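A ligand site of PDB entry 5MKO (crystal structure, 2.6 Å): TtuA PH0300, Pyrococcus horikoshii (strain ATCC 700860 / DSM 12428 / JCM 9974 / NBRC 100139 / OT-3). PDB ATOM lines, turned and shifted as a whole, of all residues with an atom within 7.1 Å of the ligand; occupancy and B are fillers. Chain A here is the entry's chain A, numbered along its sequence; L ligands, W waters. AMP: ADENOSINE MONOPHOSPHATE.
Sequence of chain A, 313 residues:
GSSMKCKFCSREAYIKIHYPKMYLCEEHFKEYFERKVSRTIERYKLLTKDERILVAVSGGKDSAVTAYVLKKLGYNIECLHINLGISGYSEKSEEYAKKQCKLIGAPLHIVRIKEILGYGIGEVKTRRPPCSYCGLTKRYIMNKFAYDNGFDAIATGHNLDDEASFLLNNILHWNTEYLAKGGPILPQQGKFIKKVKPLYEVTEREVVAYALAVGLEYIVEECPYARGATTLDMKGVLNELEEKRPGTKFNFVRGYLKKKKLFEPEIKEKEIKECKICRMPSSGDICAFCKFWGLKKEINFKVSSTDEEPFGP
O2' of the ligand sits at hydrogen-bond distance from O of Ala 56 (2.7 Å). N of Ile 82 lies within hydrogen-bond range of N1 of the ligand (2.9 Å). O of Ile 82 sits at hydrogen-bond distance from N6 of the ligand (2.8 Å). The backbone NH (N) of Gly 157 is in hydrogen-bond range of an oxygen (O3') of the ligand (3.1 Å). O1P of the ligand lies within salt-bridge range of NZ of Lys 138 (3.2 Å).
N of Ala 56 sits at hydrogen-bond distance from O of Ala 155 (3.2 Å). The backbone carbonyl oxygen (O) of Leu 80 is in hydrogen-bond range of the backbone NH (N) of Val 57, 2.8 Å away. A ring nitrogen (ND1) of His 81 is in hydrogen-bond range of the backbone carbonyl oxygen (O) of Val 57. OG of Ser 58 sits at hydrogen-bond distance from OG of Ser 63. ND1 of His 158 sits at hydrogen-bond distance from OG1 of Thr 156 (2.8 Å). The backbone NH (N) of Leu 80 is in hydrogen-bond range of the backbone carbonyl oxygen (O) of Val 55 (2.9 Å). The backbone carbonyl oxygen of His 81 lies within hydrogen-bond range of the backbone NH of Val 111.
The backbone carbonyl oxygen (O) of Val 57 sits close to a nitrogen (N1) of the ligand. Ser 58 touches the ligand. Ser 63 touches the ligand (CB to O2', 3.5 Å). Leu 80 touches the ligand. C of His 81 touches N1 of the ligand, at 3.9 Å. Leu 84 touches the ligand. Thr 156 touches the ligand. His 158 touches the ligand (CE1 to C5', 3.4 Å). 12 residues have an atom within 4 Å of the ligand: Ala 56, Val 57, Ser 58, Ser 63, Leu 80, His 81, Ile 82, Leu 84, Lys 138, Thr 156, Gly 157 and His 158. Along chain A the residues within 4 Å of the ligand span positions 56 to 158. The nearest printed residue that does not touch the ligand is Met 142 (4.2 Å).
Water W1 bridges O2P of the ligand (3.0 Å) and OD2 of Asp 162 (3.4 Å).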
ATOM      1  N   VAL A  55       9.000 -16.516 -17.700  1.00  0.00           N
ATOM      2  CA  VAL A  55       8.393 -15.193 -17.647  1.00  0.00           C
ATOM      3  C   VAL A  55       7.113 -15.197 -18.483  1.00  0.00           C
ATOM      4  O   VAL A  55       7.161 -15.420 -19.693  1.00  0.00           O
ATOM      5  CB  VAL A  55       9.353 -14.001 -17.971  1.00  0.00           C
ATOM      6  CG1 VAL A  55       8.663 -12.651 -17.689  1.00  0.00           C
ATOM      7  CG2 VAL A  55      10.655 -14.117 -17.173  1.00  0.00           C
ATOM      8  N   ALA A  56       5.968 -14.982 -17.824  1.00  0.00           N
ATOM      9  CA  ALA A  56       4.666 -14.927 -18.470  1.00  0.00           C
ATOM     10  C   ALA A  56       4.580 -13.547 -19.108  1.00  0.00           C
ATOM     11  O   ALA A  56       4.470 -12.533 -18.400  1.00  0.00           O
ATOM     12  CB  ALA A  56       3.576 -15.126 -17.428  1.00  0.00           C
ATOM     13  N   VAL A  57       4.737 -13.478 -20.435  1.00  0.00           N
ATOM     14  CA  VAL A  57       4.750 -12.212 -21.195  1.00  0.00           C
ATOM     15  C   VAL A  57       3.401 -11.978 -21.883  1.00  0.00           C
ATOM     16  O   VAL A  57       2.944 -12.791 -22.675  1.00  0.00           O
ATOM     17  CB  VAL A  57       5.969 -12.069 -22.146  1.00  0.00           C
ATOM     18  CG1 VAL A  57       7.286 -12.082 -21.370  1.00  0.00           C
ATOM     19  CG2 VAL A  57       5.987 -13.139 -23.228  1.00  0.00           C
ATOM     20  N   SER A  58       2.759 -10.861 -21.537  1.00  0.00           N
ATOM     21  CA  SER A  58       1.434 -10.479 -22.030  1.00  0.00           C
ATOM     22  C   SER A  58       1.445  -9.667 -23.326  1.00  0.00           C
ATOM     23  O   SER A  58       0.437  -9.664 -24.047  1.00  0.00           O
ATOM     24  CB  SER A  58       0.704  -9.659 -20.972  1.00  0.00           C
ATOM     25  OG  SER A  58       1.518  -8.607 -20.481  1.00  0.00           O
ATOM     26  N   GLY A  59       2.546  -8.974 -23.581  1.00  0.00           N
ATOM     27  CA  GLY A  59       2.695  -8.042 -24.689  1.00  0.00           C
ATOM     28  C   GLY A  59       2.744  -6.620 -24.156  1.00  0.00           C
ATOM     29  O   GLY A  59       3.081  -5.695 -24.892  1.00  0.00           O
ATOM     30  N   ASP A  62       5.056  -4.293 -18.407  1.00  0.00           N
ATOM     31  CA  ASP A  62       5.406  -4.926 -17.146  1.00  0.00           C
ATOM     32  C   ASP A  62       6.144  -6.251 -17.302  1.00  0.00           C
ATOM     33  O   ASP A  62       7.282  -6.366 -16.832  1.00  0.00           O
ATOM     34  CB  ASP A  62       4.153  -5.059 -16.270  1.00  0.00           C
ATOM     35  CG  ASP A  62       3.427  -3.736 -16.084  1.00  0.00           C
ATOM     36  OD1 ASP A  62       3.916  -2.896 -15.309  1.00  0.00           O
ATOM     37  OD2 ASP A  62       2.396  -3.524 -16.779  1.00  0.00           O
ATOM     38  N   SER A  63       5.543  -7.226 -17.990  1.00  0.00           N
ATOM     39  CA  SER A  63       6.163  -8.534 -18.231  1.00  0.00           C
ATOM     40  C   SER A  63       7.373  -8.455 -19.180  1.00  0.00           C
ATOM     41  O   SER A  63       8.289  -9.271 -19.067  1.00  0.00           O
ATOM     42  CB  SER A  63       5.130  -9.511 -18.776  1.00  0.00           C
ATOM     43  OG  SER A  63       4.343  -8.948 -19.821  1.00  0.00           O
ATOM     44  N   ALA A  64       7.366  -7.462 -20.110  1.00  0.00           N
ATOM     45  CA  ALA A  64       8.453  -7.202 -21.053  1.00  0.00           C
ATOM     46  C   ALA A  64       9.687  -6.718 -20.301  1.00  0.00           C
ATOM     47  O   ALA A  64      10.799  -7.164 -20.585  1.00  0.00           O
ATOM     48  CB  ALA A  64       8.026  -6.154 -22.055  1.00  0.00           C
ATOM     49  N   THR A  66      10.121  -7.160 -16.992  1.00  0.00           N
ATOM     50  CA  THR A  66      10.472  -8.246 -16.059  1.00  0.00           C
ATOM     51  C   THR A  66      11.489  -9.159 -16.743  1.00  0.00           C
ATOM     52  O   THR A  66      12.575  -9.376 -16.210  1.00  0.00           O
ATOM     53  CB  THR A  66       9.223  -9.026 -15.596  1.00  0.00           C
ATOM     54  OG1 THR A  66       8.279  -8.121 -15.037  1.00  0.00           O
ATOM     55  CG2 THR A  66       9.551 -10.123 -14.584  1.00  0.00           C
ATOM     56  N   LEU A  80       6.688 -17.177 -21.894  1.00  0.00           N
ATOM     57  CA  LEU A  80       5.423 -17.733 -22.344  1.00  0.00           C
ATOM     58  C   LEU A  80       4.410 -16.651 -22.656  1.00  0.00           C
ATOM     59  O   LEU A  80       4.167 -15.789 -21.823  1.00  0.00           O
ATOM     60  CB  LEU A  80       4.836 -18.780 -21.369  1.00  0.00           C
ATOM     61  CG  LEU A  80       3.401 -19.297 -21.687  1.00  0.00           C
ATOM     62  CD1 LEU A  80       3.360 -20.171 -22.914  1.00  0.00           C
ATOM     63  CD2 LEU A  80       2.798 -20.026 -20.517  1.00  0.00           C
ATOM     64  N   HIS A  81       3.829 -16.696 -23.855  1.00  0.00           N
ATOM     65  CA  HIS A  81       2.767 -15.801 -24.235  1.00  0.00           C
ATOM     66  C   HIS A  81       1.523 -16.629 -24.495  1.00  0.00           C
ATOM     67  O   HIS A  81       1.578 -17.618 -25.230  1.00  0.00           O
ATOM     68  CB  HIS A  81       3.119 -14.933 -25.456  1.00  0.00           C
ATOM     69  CG  HIS A  81       1.966 -14.091 -25.924  1.00  0.00           C
ATOM     70  ND1 HIS A  81       1.542 -12.998 -25.195  1.00  0.00           N
ATOM     71  CD2 HIS A  81       1.138 -14.273 -26.984  1.00  0.00           C
ATOM     72  CE1 HIS A  81       0.477 -12.534 -25.842  1.00  0.00           C
ATOM     73  NE2 HIS A  81       0.200 -13.262 -26.919  1.00  0.00           N
ATOM     74  N   ILE A  82       0.408 -16.241 -23.874  1.00  0.00           N
ATOM     75  CA  ILE A  82      -0.873 -16.927 -24.062  1.00  0.00           C
ATOM     76  C   ILE A  82      -1.773 -16.053 -24.926  1.00  0.00           C
ATOM     77  O   ILE A  82      -2.107 -14.938 -24.548  1.00  0.00           O
ATOM     78  CB  ILE A  82      -1.545 -17.370 -22.728  1.00  0.00           C
ATOM     79  CG1 ILE A  82      -0.517 -17.987 -21.731  1.00  0.00           C
ATOM     80  CG2 ILE A  82      -2.710 -18.346 -23.013  1.00  0.00           C
ATOM     81  CD1 ILE A  82      -0.927 -17.963 -20.284  1.00  0.00           C
ATOM     82  N   ASN A  83      -2.105 -16.529 -26.134  1.00  0.00           N
ATOM     83  CA  ASN A  83      -2.979 -15.851 -27.077  1.00  0.00           C
ATOM     84  C   ASN A  83      -4.401 -16.280 -26.728  1.00  0.00           C
ATOM     85  O   ASN A  83      -4.767 -17.454 -26.915  1.00  0.00           O
ATOM     86  CB  ASN A  83      -2.614 -16.238 -28.517  1.00  0.00           C
ATOM     87  CG  ASN A  83      -3.370 -15.513 -29.591  1.00  0.00           C
ATOM     88  OD1 ASN A  83      -4.591 -15.681 -29.766  1.00  0.00           O
ATOM     89  ND2 ASN A  83      -2.669 -14.734 -30.394  1.00  0.00           N
ATOM     90  N   LEU A  84      -5.202 -15.350 -26.182  1.00  0.00           N
ATOM     91  CA  LEU A  84      -6.567 -15.605 -25.748  1.00  0.00           C
ATOM     92  C   LEU A  84      -7.601 -15.586 -26.902  1.00  0.00           C
ATOM     93  O   LEU A  84      -8.806 -15.617 -26.645  1.00  0.00           O
ATOM     94  CB  LEU A  84      -7.012 -14.665 -24.605  1.00  0.00           C
ATOM     95  CG  LEU A  84      -6.130 -14.520 -23.338  1.00  0.00           C
ATOM     96  CD1 LEU A  84      -5.676 -15.861 -22.729  1.00  0.00           C
ATOM     97  CD2 LEU A  84      -5.028 -13.536 -23.534  1.00  0.00           C
ATOM     98  N   SER A  93      -0.985  -8.303 -29.703  1.00  0.00           N
ATOM     99  CA  SER A  93      -0.345  -8.669 -28.435  1.00  0.00           C
ATOM    100  C   SER A  93       0.695  -9.771 -28.619  1.00  0.00           C
ATOM    101  O   SER A  93       1.739  -9.721 -27.962  1.00  0.00           O
ATOM    102  CB  SER A  93      -1.396  -9.073 -27.405  1.00  0.00           C
ATOM    103  OG  SER A  93      -2.251  -7.973 -27.092  1.00  0.00           O
ATOM    104  N   VAL A 111       1.168 -20.158 -26.679  1.00  0.00           N
ATOM    105  CA  VAL A 111       0.024 -21.042 -26.499  1.00  0.00           C
ATOM    106  C   VAL A 111      -1.239 -20.290 -26.972  1.00  0.00           C
ATOM    107  O   VAL A 111      -1.584 -19.240 -26.434  1.00  0.00           O
ATOM    108  CB  VAL A 111      -0.102 -21.577 -25.032  1.00  0.00           C
ATOM    109  CG1 VAL A 111      -1.424 -22.305 -24.822  1.00  0.00           C
ATOM    110  CG2 VAL A 111       1.072 -22.478 -24.676  1.00  0.00           C
ATOM    111  N   CYS A 134     -10.963 -15.303 -17.780  1.00  0.00           N
ATOM    112  CA  CYS A 134      -9.720 -14.895 -18.425  1.00  0.00           C
ATOM    113  C   CYS A 134      -8.563 -15.247 -17.491  1.00  0.00           C
ATOM    114  O   CYS A 134      -7.674 -16.021 -17.878  1.00  0.00           O
ATOM    115  CB  CYS A 134      -9.750 -13.401 -18.734  1.00  0.00           C
ATOM    116  SG  CYS A 134      -8.192 -12.696 -19.303  1.00  0.00           S
ATOM    117  N   GLY A 135      -8.612 -14.714 -16.268  1.00  0.00           N
ATOM    118  CA  GLY A 135      -7.623 -14.916 -15.212  1.00  0.00           C
ATOM    119  C   GLY A 135      -7.453 -16.373 -14.832  1.00  0.00           C
ATOM    120  O   GLY A 135      -6.331 -16.819 -14.615  1.00  0.00           O
ATOM    121  N   LYS A 138      -5.523 -17.971 -17.903  1.00  0.00           N
ATOM    122  CA  LYS A 138      -4.109 -17.564 -17.913  1.00  0.00           C
ATOM    123  C   LYS A 138      -3.299 -18.221 -16.797  1.00  0.00           C
ATOM    124  O   LYS A 138      -2.266 -18.818 -17.076  1.00  0.00           O
ATOM    125  CB  LYS A 138      -3.944 -16.040 -17.883  1.00  0.00           C
ATOM    126  CG  LYS A 138      -4.363 -15.363 -19.182  1.00  0.00           C
ATOM    127  CD  LYS A 138      -4.078 -13.864 -19.202  1.00  0.00           C
ATOM    128  CE  LYS A 138      -4.843 -13.043 -18.181  1.00  0.00           C
ATOM    129  NZ  LYS A 138      -4.636 -11.594 -18.389  1.00  0.00           N
ATOM    130  N   ARG A 139      -3.776 -18.105 -15.543  1.00  0.00           N
ATOM    131  CA  ARG A 139      -3.140 -18.646 -14.335  1.00  0.00           C
ATOM    132  C   ARG A 139      -2.910 -20.159 -14.410  1.00  0.00           C
ATOM    133  O   ARG A 139      -1.872 -20.617 -13.923  1.00  0.00           O
ATOM    134  CB  ARG A 139      -3.949 -18.273 -13.073  1.00  0.00           C
ATOM    135  CG  ARG A 139      -3.516 -16.953 -12.440  1.00  0.00           C
ATOM    136  CD  ARG A 139      -4.442 -16.511 -11.313  1.00  0.00           C
ATOM    137  NE  ARG A 139      -5.466 -15.581 -11.804  1.00  0.00           N
ATOM    138  CZ  ARG A 139      -6.665 -15.431 -11.252  1.00  0.00           C
ATOM    139  NH1 ARG A 139      -7.011 -16.150 -10.188  1.00  0.00           N
ATOM    140  NH2 ARG A 139      -7.534 -14.576 -11.769  1.00  0.00           N
ATOM    141  N   MET A 142      -0.341 -20.941 -17.533  1.00  0.00           N
ATOM    142  CA  MET A 142       1.035 -20.604 -17.170  1.00  0.00           C
ATOM    143  C   MET A 142       1.568 -21.539 -16.088  1.00  0.00           C
ATOM    144  O   MET A 142       2.760 -21.827 -16.127  1.00  0.00           O
ATOM    145  CB  MET A 142       1.270 -19.114 -16.840  1.00  0.00           C
ATOM    146  CG  MET A 142       0.660 -18.615 -15.554  1.00  0.00           C
ATOM    147  SD  MET A 142       0.934 -16.845 -15.277  1.00  0.00           S
ATOM    148  CE  MET A 142      -0.368 -16.133 -16.318  1.00  0.00           C
ATOM    149  N   ALA A 155       7.636 -15.922 -13.229  1.00  0.00           N
ATOM    150  CA  ALA A 155       7.771 -14.514 -12.884  1.00  0.00           C
ATOM    151  C   ALA A 155       6.749 -13.702 -13.671  1.00  0.00           C
ATOM    152  O   ALA A 155       6.606 -13.894 -14.893  1.00  0.00           O
ATOM    153  CB  ALA A 155       9.190 -14.029 -13.162  1.00  0.00           C
ATOM    154  N   THR A 156       5.996 -12.846 -12.963  1.00  0.00           N
ATOM    155  CA  THR A 156       4.983 -11.994 -13.563  1.00  0.00           C
ATOM    156  C   THR A 156       5.424 -10.534 -13.508  1.00  0.00           C
ATOM    157  O   THR A 156       6.396 -10.214 -12.820  1.00  0.00           O
ATOM    158  CB  THR A 156       3.584 -12.268 -12.979  1.00  0.00           C
ATOM    159  OG1 THR A 156       3.601 -12.075 -11.555  1.00  0.00           O
ATOM    160  CG2 THR A 156       3.042 -13.635 -13.358  1.00  0.00           C
ATOM    161  N   GLY A 157       4.723  -9.682 -14.248  1.00  0.00           N
ATOM    162  CA  GLY A 157       5.024  -8.250 -14.365  1.00  0.00           C
ATOM    163  C   GLY A 157       4.471  -7.321 -13.310  1.00  0.00           C
ATOM    164  O   GLY A 157       4.686  -6.113 -13.412  1.00  0.00           O
ATOM    165  N   HIS A 158       3.780  -7.847 -12.271  1.00  0.00           N
ATOM    166  CA  HIS A 158       3.172  -7.034 -11.194  1.00  0.00           C
ATOM    167  C   HIS A 158       4.158  -6.072 -10.512  1.00  0.00           C
ATOM    168  O   HIS A 158       5.155  -6.495  -9.917  1.00  0.00           O
ATOM    169  CB  HIS A 158       2.508  -7.904 -10.134  1.00  0.00           C
ATOM    170  CG  HIS A 158       1.435  -8.800 -10.663  1.00  0.00           C
ATOM    171  ND1 HIS A 158       1.727 -10.019 -11.221  1.00  0.00           N
ATOM    172  CD2 HIS A 158       0.098  -8.651 -10.616  1.00  0.00           C
ATOM    173  CE1 HIS A 158       0.564 -10.574 -11.503  1.00  0.00           C
ATOM    174  NE2 HIS A 158      -0.454  -9.783 -11.166  1.00  0.00           N
ATOM    175  N   ASN A 159       3.859  -4.765 -10.639  1.00  0.00           N
ATOM    176  CA  ASN A 159       4.644  -3.676 -10.076  1.00  0.00           C
ATOM    177  C   ASN A 159       4.071  -3.200  -8.720  1.00  0.00           C
ATOM    178  O   ASN A 159       3.066  -3.757  -8.252  1.00  0.00           O
ATOM    179  CB  ASN A 159       4.785  -2.511 -11.096  1.00  0.00           C
ATOM    180  CG  ASN A 159       3.491  -1.919 -11.605  1.00  0.00           C
ATOM    181  OD1 ASN A 159       2.520  -1.706 -10.861  1.00  0.00           O
ATOM    182  ND2 ASN A 159       3.457  -1.559 -12.880  1.00  0.00           N
ATOM    183  N   ASP A 162       0.388  -2.078  -8.807  1.00  0.00           N
ATOM    184  CA  ASP A 162      -0.517  -3.235  -8.879  1.00  0.00           C
ATOM    185  C   ASP A 162      -0.802  -3.798  -7.493  1.00  0.00           C
ATOM    186  O   ASP A 162      -1.950  -4.092  -7.175  1.00  0.00           O
ATOM    187  CB  ASP A 162       0.050  -4.338  -9.802  1.00  0.00           C
ATOM    188  CG  ASP A 162       0.168  -3.957 -11.268  1.00  0.00           C
ATOM    189  OD1 ASP A 162      -0.795  -3.352 -11.810  1.00  0.00           O
ATOM    190  OD2 ASP A 162       1.203  -4.315 -11.896  1.00  0.00           O
HETATM  191  P   AMP L   1      -3.003  -9.164 -15.531  1.00  0.00           P
HETATM  192  O1P AMP L   1      -3.509  -8.916 -16.978  1.00  0.00           O
HETATM  193  O2P AMP L   1      -2.599  -7.803 -14.877  1.00  0.00           O
HETATM  194  O3P AMP L   1      -3.913 -10.000 -14.698  1.00  0.00           O
HETATM  195  O5' AMP L   1      -1.650  -9.953 -15.700  1.00  0.00           O
HETATM  196  C5' AMP L   1      -0.722 -10.223 -14.628  1.00  0.00           C
HETATM  197  C4' AMP L   1       0.530 -10.807 -15.231  1.00  0.00           C
HETATM  198  O4' AMP L   1       0.192 -11.998 -15.979  1.00  0.00           O
HETATM  199  C3' AMP L   1       1.223  -9.901 -16.238  1.00  0.00           C
HETATM  200  O3' AMP L   1       2.043  -8.955 -15.574  1.00  0.00           O
HETATM  201  C2' AMP L   1       1.986 -10.905 -17.089  1.00  0.00           C
HETATM  202  O2' AMP L   1       3.183 -11.313 -16.425  1.00  0.00           O
HETATM  203  C1' AMP L   1       1.009 -12.100 -17.130  1.00  0.00           C
HETATM  204  N9  AMP L   1       0.151 -12.167 -18.315  1.00  0.00           N
HETATM  205  C8  AMP L   1      -1.004 -11.465 -18.548  1.00  0.00           C
HETATM  206  N7  AMP L   1      -1.574 -11.739 -19.693  1.00  0.00           N
HETATM  207  C5  AMP L   1      -0.747 -12.685 -20.265  1.00  0.00           C
HETATM  208  C6  AMP L   1      -0.788 -13.376 -21.489  1.00  0.00           C
HETATM  209  N6  AMP L   1      -1.706 -13.154 -22.439  1.00  0.00           N
HETATM  210  N1  AMP L   1       0.192 -14.284 -21.740  1.00  0.00           N
HETATM  211  C2  AMP L   1       1.146 -14.462 -20.831  1.00  0.00           C
HETATM  212  N3  AMP L   1       1.309 -13.853 -19.648  1.00  0.00           N
HETATM  213  C4  AMP L   1       0.320 -12.967 -19.423  1.00  0.00           C
HETATM  214  O   HOH W   1      -0.132  -6.264 -14.377  1.00  0.00           O
